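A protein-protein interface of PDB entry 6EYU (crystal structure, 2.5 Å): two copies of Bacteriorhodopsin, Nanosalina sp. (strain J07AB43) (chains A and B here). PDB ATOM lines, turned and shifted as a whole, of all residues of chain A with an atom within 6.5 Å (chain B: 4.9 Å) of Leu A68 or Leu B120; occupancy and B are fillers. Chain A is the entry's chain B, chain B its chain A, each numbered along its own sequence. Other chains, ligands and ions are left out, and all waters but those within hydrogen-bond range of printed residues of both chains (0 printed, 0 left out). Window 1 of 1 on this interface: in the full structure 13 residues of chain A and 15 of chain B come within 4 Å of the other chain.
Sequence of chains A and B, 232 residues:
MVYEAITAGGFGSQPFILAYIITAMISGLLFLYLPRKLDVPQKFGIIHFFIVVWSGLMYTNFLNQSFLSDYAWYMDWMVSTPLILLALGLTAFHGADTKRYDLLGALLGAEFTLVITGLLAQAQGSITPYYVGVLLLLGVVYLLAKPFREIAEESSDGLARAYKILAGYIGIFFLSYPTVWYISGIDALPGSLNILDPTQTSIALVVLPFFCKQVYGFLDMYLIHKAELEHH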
ATOM      1  N   LEU A  57     -15.019  15.464 -11.607  1.00  0.00           N
ATOM      2  CA  LEU A  57     -15.167  14.024 -11.448  1.00  0.00           C
ATOM      3  C   LEU A  57     -14.137  13.481 -10.463  1.00  0.00           C
ATOM      4  O   LEU A  57     -14.451  12.632  -9.630  1.00  0.00           O
ATOM      5  CB  LEU A  57     -15.019  13.320 -12.797  1.00  0.00           C
ATOM      6  CG  LEU A  57     -16.302  13.247 -13.628  1.00  0.00           C
ATOM      7  CD1 LEU A  57     -15.982  12.971 -15.089  1.00  0.00           C
ATOM      8  CD2 LEU A  57     -17.240  12.188 -13.069  1.00  0.00           C
ATOM      9  N   MET A  58     -12.918  14.007 -10.537  1.00  0.00           N
ATOM     10  CA  MET A  58     -11.842  13.554  -9.662  1.00  0.00           C
ATOM     11  C   MET A  58     -12.122  13.952  -8.216  1.00  0.00           C
ATOM     12  O   MET A  58     -11.682  13.279  -7.284  1.00  0.00           O
ATOM     13  CB  MET A  58     -10.503  14.143 -10.112  1.00  0.00           C
ATOM     14  CG  MET A  58     -10.005  13.615 -11.449  1.00  0.00           C
ATOM     15  SD  MET A  58     -10.453  11.893 -11.745  1.00  0.00           S
ATOM     16  CE  MET A  58      -9.710  11.096 -10.323  1.00  0.00           C
ATOM     17  N   THR A  60     -14.908  14.003  -6.710  1.00  0.00           N
ATOM     18  CA  THR A  60     -15.909  13.127  -6.110  1.00  0.00           C
ATOM     19  C   THR A  60     -15.248  12.052  -5.252  1.00  0.00           C
ATOM     20  O   THR A  60     -15.928  11.304  -4.551  1.00  0.00           O
ATOM     21  CB  THR A  60     -16.775  12.441  -7.183  1.00  0.00           C
ATOM     22  OG1 THR A  60     -15.947  11.636  -8.031  1.00  0.00           O
ATOM     23  CG2 THR A  60     -17.508  13.476  -8.023  1.00  0.00           C
ATOM     24  N   ASN A  61     -13.922  11.979  -5.312  1.00  0.00           N
ATOM     25  CA  ASN A  61     -13.179  10.994  -4.534  1.00  0.00           C
ATOM     26  C   ASN A  61     -12.916  11.501  -3.118  1.00  0.00           C
ATOM     27  O   ASN A  61     -12.397  10.769  -2.276  1.00  0.00           O
ATOM     28  CB  ASN A  61     -11.852  10.659  -5.219  1.00  0.00           C
ATOM     29  CG  ASN A  61     -12.033   9.776  -6.438  1.00  0.00           C
ATOM     30  OD1 ASN A  61     -12.474   8.632  -6.330  1.00  0.00           O
ATOM     31  ND2 ASN A  61     -11.667  10.295  -7.604  1.00  0.00           N
ATOM     32  N   GLN A  65     -14.889   7.671  -0.639  1.00  0.00           N
ATOM     33  CA  GLN A  65     -13.532   7.159  -0.514  1.00  0.00           C
ATOM     34  C   GLN A  65     -13.262   6.088  -1.562  1.00  0.00           C
ATOM     35  O   GLN A  65     -14.075   5.186  -1.772  1.00  0.00           O
ATOM     36  CB  GLN A  65     -13.297   6.587   0.883  1.00  0.00           C
ATOM     37  CG  GLN A  65     -12.083   5.677   0.973  1.00  0.00           C
ATOM     38  CD  GLN A  65     -11.443   5.691   2.346  1.00  0.00           C
ATOM     39  OE1 GLN A  65     -10.355   6.236   2.531  1.00  0.00           O
ATOM     40  NE2 GLN A  65     -12.128   5.110   3.323  1.00  0.00           N
ATOM     41  N   SER A  66     -12.083   6.157  -2.167  1.00  0.00           N
ATOM     42  CA  SER A  66     -11.616   5.115  -3.071  1.00  0.00           C
ATOM     43  C   SER A  66     -10.097   5.028  -2.981  1.00  0.00           C
ATOM     44  O   SER A  66      -9.468   5.807  -2.265  1.00  0.00           O
ATOM     45  CB  SER A  66     -12.037   5.435  -4.507  1.00  0.00           C
ATOM     46  OG  SER A  66     -11.449   6.645  -4.951  1.00  0.00           O
ATOM     47  N   PHE A  67      -9.509   4.079  -3.701  1.00  0.00           N
ATOM     48  CA  PHE A  67      -8.061   3.913  -3.684  1.00  0.00           C
ATOM     49  C   PHE A  67      -7.377   5.115  -4.326  1.00  0.00           C
ATOM     50  O   PHE A  67      -6.166   5.296  -4.184  1.00  0.00           O
ATOM     51  CB  PHE A  67      -7.659   2.628  -4.410  1.00  0.00           C
ATOM     52  CG  PHE A  67      -7.765   2.719  -5.905  1.00  0.00           C
ATOM     53  CD1 PHE A  67      -6.687   3.139  -6.664  1.00  0.00           C
ATOM     54  CD2 PHE A  67      -8.920   2.318  -6.555  1.00  0.00           C
ATOM     55  CE1 PHE A  67      -6.787   3.242  -8.039  1.00  0.00           C
ATOM     56  CE2 PHE A  67      -9.032   2.425  -7.928  1.00  0.00           C
ATOM     57  CZ  PHE A  67      -7.961   2.880  -8.673  1.00  0.00           C
ATOM     58  N   LEU A  68      -8.175   6.004  -4.909  1.00  0.00           N
ATOM     59  CA  LEU A  68      -7.640   7.151  -5.636  1.00  0.00           C
ATOM     60  C   LEU A  68      -7.542   8.378  -4.732  1.00  0.00           C
ATOM     61  O   LEU A  68      -6.862   9.349  -5.063  1.00  0.00           O
ATOM     62  CB  LEU A  68      -8.518   7.472  -6.849  1.00  0.00           C
ATOM     63  CG  LEU A  68      -8.436   6.485  -8.017  1.00  0.00           C
ATOM     64  CD1 LEU A  68      -9.452   6.843  -9.090  1.00  0.00           C
ATOM     65  CD2 LEU A  68      -7.030   6.451  -8.599  1.00  0.00           C
ATOM     66  N   SER A  69      -8.262   8.348  -3.615  1.00  0.00           N
ATOM     67  CA  SER A  69      -8.667   9.573  -2.933  1.00  0.00           C
ATOM     68  C   SER A  69      -7.454  10.387  -2.492  1.00  0.00           C
ATOM     69  O   SER A  69      -7.461  11.616  -2.567  1.00  0.00           O
ATOM     70  CB  SER A  69      -9.540   9.245  -1.720  1.00  0.00           C
ATOM     71  OG  SER A  69     -10.756   8.634  -2.118  1.00  0.00           O
ATOM     72  N   ASP A  70      -6.446   9.703  -1.960  1.00  0.00           N
ATOM     73  CA  ASP A  70      -5.282  10.375  -1.389  1.00  0.00           C
ATOM     74  C   ASP A  70      -4.539  11.165  -2.461  1.00  0.00           C
ATOM     75  O   ASP A  70      -3.833  12.128  -2.160  1.00  0.00           O
ATOM     76  CB  ASP A  70      -4.339   9.357  -0.748  1.00  0.00           C
ATOM     77  CG  ASP A  70      -4.888   8.785   0.545  1.00  0.00           C
ATOM     78  OD1 ASP A  70      -5.431   9.564   1.356  1.00  0.00           O
ATOM     79  OD2 ASP A  70      -4.755   7.562   0.759  1.00  0.00           O
ATOM     80  N   TYR A  71      -4.677  10.730  -3.709  1.00  0.00           N
ATOM     81  CA  TYR A  71      -3.919  11.311  -4.809  1.00  0.00           C
ATOM     82  C   TYR A  71      -4.868  11.931  -5.829  1.00  0.00           C
ATOM     83  O   TYR A  71      -4.478  12.209  -6.964  1.00  0.00           O
ATOM     84  CB  TYR A  71      -3.047  10.242  -5.471  1.00  0.00           C
ATOM     85  CG  TYR A  71      -2.012   9.640  -4.544  1.00  0.00           C
ATOM     86  CD1 TYR A  71      -0.798  10.278  -4.323  1.00  0.00           C
ATOM     87  CD2 TYR A  71      -2.303   8.511  -3.788  1.00  0.00           C
ATOM     88  CE1 TYR A  71       0.122   9.774  -3.422  1.00  0.00           C
ATOM     89  CE2 TYR A  71      -1.394   8.007  -2.876  1.00  0.00           C
ATOM     90  CZ  TYR A  71      -0.184   8.640  -2.700  1.00  0.00           C
ATOM     91  OH  TYR A  71       0.733   8.129  -1.809  1.00  0.00           O
ATOM     92  N   ALA A  72      -6.043  12.328  -5.351  1.00  0.00           N
ATOM     93  CA  ALA A  72      -7.086  12.871  -6.213  1.00  0.00           C
ATOM     94  C   ALA A  72      -6.606  14.139  -6.913  1.00  0.00           C
ATOM     95  O   ALA A  72      -6.738  14.271  -8.131  1.00  0.00           O
ATOM     96  CB  ALA A  72      -8.339  13.162  -5.401  1.00  0.00           C
ATOM     97  N   TRP A  73      -6.156  15.112  -6.127  1.00  0.00           N
ATOM     98  CA  TRP A  73      -5.664  16.369  -6.681  1.00  0.00           C
ATOM     99  C   TRP A  73      -4.813  16.094  -7.915  1.00  0.00           C
ATOM    100  O   TRP A  73      -4.961  16.756  -8.944  1.00  0.00           O
ATOM    101  CB  TRP A  73      -4.833  17.127  -5.644  1.00  0.00           C
ATOM    102  CG  TRP A  73      -5.624  17.614  -4.469  1.00  0.00           C
ATOM    103  CD1 TRP A  73      -6.866  18.180  -4.495  1.00  0.00           C
ATOM    104  CD2 TRP A  73      -5.156  17.746  -3.121  1.00  0.00           C
ATOM    105  NE1 TRP A  73      -7.243  18.554  -3.228  1.00  0.00           N
ATOM    106  CE2 TRP A  73      -6.216  18.280  -2.362  1.00  0.00           C
ATOM    107  CE3 TRP A  73      -3.972  17.390  -2.468  1.00  0.00           C
ATOM    108  CZ2 TRP A  73      -6.120  18.488  -0.988  1.00  0.00           C
ATOM    109  CZ3 TRP A  73      -3.881  17.592  -1.103  1.00  0.00           C
ATOM    110  CH2 TRP A  73      -4.947  18.137  -0.378  1.00  0.00           C
ATOM    111  N   MET A  75      -4.518  13.264  -9.732  1.00  0.00           N
ATOM    112  CA  MET A  75      -5.335  12.636 -10.763  1.00  0.00           C
ATOM    113  C   MET A  75      -6.087  13.699 -11.556  1.00  0.00           C
ATOM    114  O   MET A  75      -6.217  13.600 -12.777  1.00  0.00           O
ATOM    115  CB  MET A  75      -6.328  11.656 -10.136  1.00  0.00           C
ATOM    116  CG  MET A  75      -5.694  10.377  -9.612  1.00  0.00           C
ATOM    117  SD  MET A  75      -4.267   9.853 -10.582  1.00  0.00           S
ATOM    118  CE  MET A  75      -5.068   9.224 -12.055  1.00  0.00           C
ATOM    119  N   ILE B 116     -13.534   6.398 -17.519  1.00  0.00           N
ATOM    120  CA  ILE B 116     -12.967   6.672 -16.202  1.00  0.00           C
ATOM    121  C   ILE B 116     -14.058   6.807 -15.144  1.00  0.00           C
ATOM    122  O   ILE B 116     -13.840   6.487 -13.976  1.00  0.00           O
ATOM    123  CB  ILE B 116     -12.111   7.953 -16.198  1.00  0.00           C
ATOM    124  CG1 ILE B 116     -10.855   7.750 -17.047  1.00  0.00           C
ATOM    125  CG2 ILE B 116     -11.710   8.309 -14.774  1.00  0.00           C
ATOM    126  CD1 ILE B 116     -10.108   6.477 -16.720  1.00  0.00           C
ATOM    127  N   THR B 117     -15.236   7.266 -15.556  1.00  0.00           N
ATOM    128  CA  THR B 117     -16.387   7.298 -14.660  1.00  0.00           C
ATOM    129  C   THR B 117     -16.732   5.891 -14.184  1.00  0.00           C
ATOM    130  O   THR B 117     -16.952   5.664 -12.995  1.00  0.00           O
ATOM    131  CB  THR B 117     -17.627   7.907 -15.343  1.00  0.00           C
ATOM    132  OG1 THR B 117     -18.068   7.045 -16.400  1.00  0.00           O
ATOM    133  CG2 THR B 117     -17.309   9.282 -15.909  1.00  0.00           C
ATOM    134  N   GLY B 118     -16.755   4.944 -15.118  1.00  0.00           N
ATOM    135  CA  GLY B 118     -16.971   3.542 -14.781  1.00  0.00           C
ATOM    136  C   GLY B 118     -16.012   3.060 -13.711  1.00  0.00           C
ATOM    137  O   GLY B 118     -16.394   2.314 -12.808  1.00  0.00           O
ATOM    138  N   LEU B 119     -14.756   3.480 -13.821  1.00  0.00           N
ATOM    139  CA  LEU B 119     -13.713   3.059 -12.894  1.00  0.00           C
ATOM    140  C   LEU B 119     -13.890   3.750 -11.546  1.00  0.00           C
ATOM    141  O   LEU B 119     -13.757   3.124 -10.494  1.00  0.00           O
ATOM    142  CB  LEU B 119     -12.338   3.393 -13.476  1.00  0.00           C
ATOM    143  CG  LEU B 119     -11.121   3.080 -12.604  1.00  0.00           C
ATOM    144  CD1 LEU B 119      -9.914   2.792 -13.484  1.00  0.00           C
ATOM    145  CD2 LEU B 119     -10.831   4.234 -11.656  1.00  0.00           C
ATOM    146  N   LEU B 120     -14.285   5.018 -11.589  1.00  0.00           N
ATOM    147  CA  LEU B 120     -14.588   5.769 -10.378  1.00  0.00           C
ATOM    148  C   LEU B 120     -15.780   5.156  -9.652  1.00  0.00           C
ATOM    149  O   LEU B 120     -15.747   4.964  -8.436  1.00  0.00           O
ATOM    150  CB  LEU B 120     -14.886   7.231 -10.720  1.00  0.00           C
ATOM    151  CG  LEU B 120     -13.700   8.060 -11.217  1.00  0.00           C
ATOM    152  CD1 LEU B 120     -14.097   9.521 -11.358  1.00  0.00           C
ATOM    153  CD2 LEU B 120     -12.509   7.913 -10.284  1.00  0.00           C
ATOM    154  N   ALA B 121     -16.829   4.842 -10.405  1.00  0.00           N
ATOM    155  CA  ALA B 121     -18.031   4.247  -9.832  1.00  0.00           C
ATOM    156  C   ALA B 121     -17.680   2.998  -9.032  1.00  0.00           C
ATOM    157  O   ALA B 121     -17.999   2.901  -7.846  1.00  0.00           O
ATOM    158  CB  ALA B 121     -19.028   3.911 -10.929  1.00  0.00           C
ATOM    159  N   GLN B 122     -16.968   2.071  -9.665  1.00  0.00           N
ATOM    160  CA  GLN B 122     -16.558   0.840  -8.998  1.00  0.00           C
ATOM    161  C   GLN B 122     -15.694   1.151  -7.781  1.00  0.00           C
ATOM    162  O   GLN B 122     -15.876   0.567  -6.713  1.00  0.00           O
ATOM    163  CB  GLN B 122     -15.788  -0.064  -9.962  1.00  0.00           C
ATOM    164  CG  GLN B 122     -15.512  -1.454  -9.410  1.00  0.00           C
ATOM    165  CD  GLN B 122     -14.672  -2.300 -10.346  1.00  0.00           C
ATOM    166  OE1 GLN B 122     -15.034  -2.510 -11.504  1.00  0.00           O
ATOM    167  NE2 GLN B 122     -13.560  -2.818  -9.838  1.00  0.00           N
ATOM    168  N   ALA B 123     -14.724   2.041  -7.962  1.00  0.00           N
ATOM    169  CA  ALA B 123     -13.748   2.333  -6.918  1.00  0.00           C
ATOM    170  C   ALA B 123     -14.412   3.053  -5.749  1.00  0.00           C
ATOM    171  O   ALA B 123     -14.007   2.890  -4.599  1.00  0.00           O
ATOM    172  CB  ALA B 123     -12.611   3.170  -7.481  1.00  0.00           C
ATOM    173  N   GLN B 124     -15.474   3.798  -6.043  1.00  0.00           N
ATOM    174  CA  GLN B 124     -16.152   4.598  -5.028  1.00  0.00           C
ATOM    175  C   GLN B 124     -17.294   3.814  -4.388  1.00  0.00           C
ATOM    176  O   GLN B 124     -17.840   4.225  -3.364  1.00  0.00           O
ATOM    177  CB  GLN B 124     -16.694   5.890  -5.642  1.00  0.00           C
ATOM    178  CG  GLN B 124     -15.624   6.923  -5.960  1.00  0.00           C
ATOM    179  CD  GLN B 124     -16.206   8.222  -6.481  1.00  0.00           C
ATOM    180  OE1 GLN B 124     -17.377   8.527  -6.253  1.00  0.00           O
ATOM    181  NE2 GLN B 124     -15.390   8.992  -7.190  1.00  0.00           N
ATOM    182  N   GLY B 125     -17.724   2.748  -5.056  1.00  0.00           N
ATOM    183  CA  GLY B 125     -18.981   2.090  -4.719  1.00  0.00           C
ATOM    184  C   GLY B 125     -20.163   3.031  -4.833  1.00  0.00           C
ATOM    185  O   GLY B 125     -21.131   2.922  -4.080  1.00  0.00           O
ATOM    186  N   PRO B 129     -20.904   8.739 -10.653  1.00  0.00           N
ATOM    187  CA  PRO B 129     -20.052   8.933 -11.825  1.00  0.00           C
ATOM    188  C   PRO B 129     -20.581   8.197 -13.050  1.00  0.00           C
ATOM    189  O   PRO B 129     -20.546   8.734 -14.157  1.00  0.00           O
ATOM    190  CB  PRO B 129     -18.702   8.346 -11.388  1.00  0.00           C
ATOM    191  CG  PRO B 129     -18.758   8.271  -9.898  1.00  0.00           C
ATOM    192  CD  PRO B 129     -20.200   8.042  -9.566  1.00  0.00           C
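The side-chain amide nitrogen of Gln B124 is in hydrogen-bond range of the side-chain amide oxygen of Asn A61, at 3.1 Å.
NE2 of Gln B124 sits at hydrogen-bond distance from OG1 of Thr A60 (2.8 Å).
Leu A68 touches just these residues of chain B: Leu B119 and Leu B120.
Of chain A, only Leu A57 (3.6 Å), Asn A61 (3.7 Å) and Leu A68 (3.5 Å) come within 4 Å of Leu B120.
Of the printed residues of chain A, Gln B124 touches Thr A60, Asn A61 and Gln A65.
Of the printed residues of chain B, Ser A66 touches Ala B123 (3.2 Å).
Printed residues of chain B within 4 Å of Leu A57: Leu B120 (3.6 Å).
Printed residues of chain B within 4 Å of Gln A65: Ala B123 and Gln B124.
Of the printed residues of chain B, Thr A60 touches Gln B124 (2.8 Å).
Ala B121 touches none of the printed residues of chain A.
Gly B125 touches none of the printed residues of chain A.
The nearest residue of chain A that does not touch Leu B120 is Met A58 (4.2 Å).
The nearest printed residue of chain A that does not touch Leu B119 is Phe A67 (4.4 Å).
No position is printed for both chains.
Of the 11 printed residues of chain B, 4 touch a printed residue of chain A.
Printed residues of chain B that touch a printed residue of chain A: Leu B119, Leu B120, Ala B123 and Gln B124.
Hydrophobic or aromatic side chains of chain B that line the printed part of chain A: Leu B119, Leu B120 and Ala B123.
Hydrophobic or aromatic side chains of chain A that line the printed part of chain B: Phe A67 and Leu A68.
Among the printed residues, 10 pairs touch across the chains.
Among the printed residues, no Asp or Glu carboxylate lies within 4 Å of a Lys or Arg side-chain nitrogen of the other chain.
Leu A57 touches Leu B120 (O to CD1, 3.6 Å).
ND2 of Asn A61 touches CD2 of Leu B120, 3.7 Å away.
O of Gln A65 touches O of Ala B123, 3.6 Å away.
Gln B124 touches Gln A65.
CB of Ser A66 touches O of Ala B123, 3.2 Å away.
Ala B123 touches Phe A67 (CB to CE2, 3.7 Å).
Leu A68 touches Leu B119.
Leu B120 touches Leu A68 (CD2 to CD1, 3.5 Å).
The side-chain amide oxygen (OD1) of Asn A61 is in hydrogen-bond range of the side-chain hydroxyl (OG) of Ser A66, at 2.6 Å.
OG of Ser A69 is in hydrogen-bond range of N of Ser A66, 2.8 Å away.
The backbone carbonyl oxygen of Asn A61 sits at hydrogen-bond distance from the side-chain hydroxyl of Ser A69 (2.7 Å).
O of Met A58 is in hydrogen-bond range of ND2 of Asn A61, at 3.0 Å.
The side-chain hydroxyl of Thr A60 sits at hydrogen-bond distance from the backbone carbonyl oxygen of Leu A57 (2.4 Å).
The side-chain hydroxyl (OG) of Ser A66 lies close to the backbone NH (N) of Leu A68.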
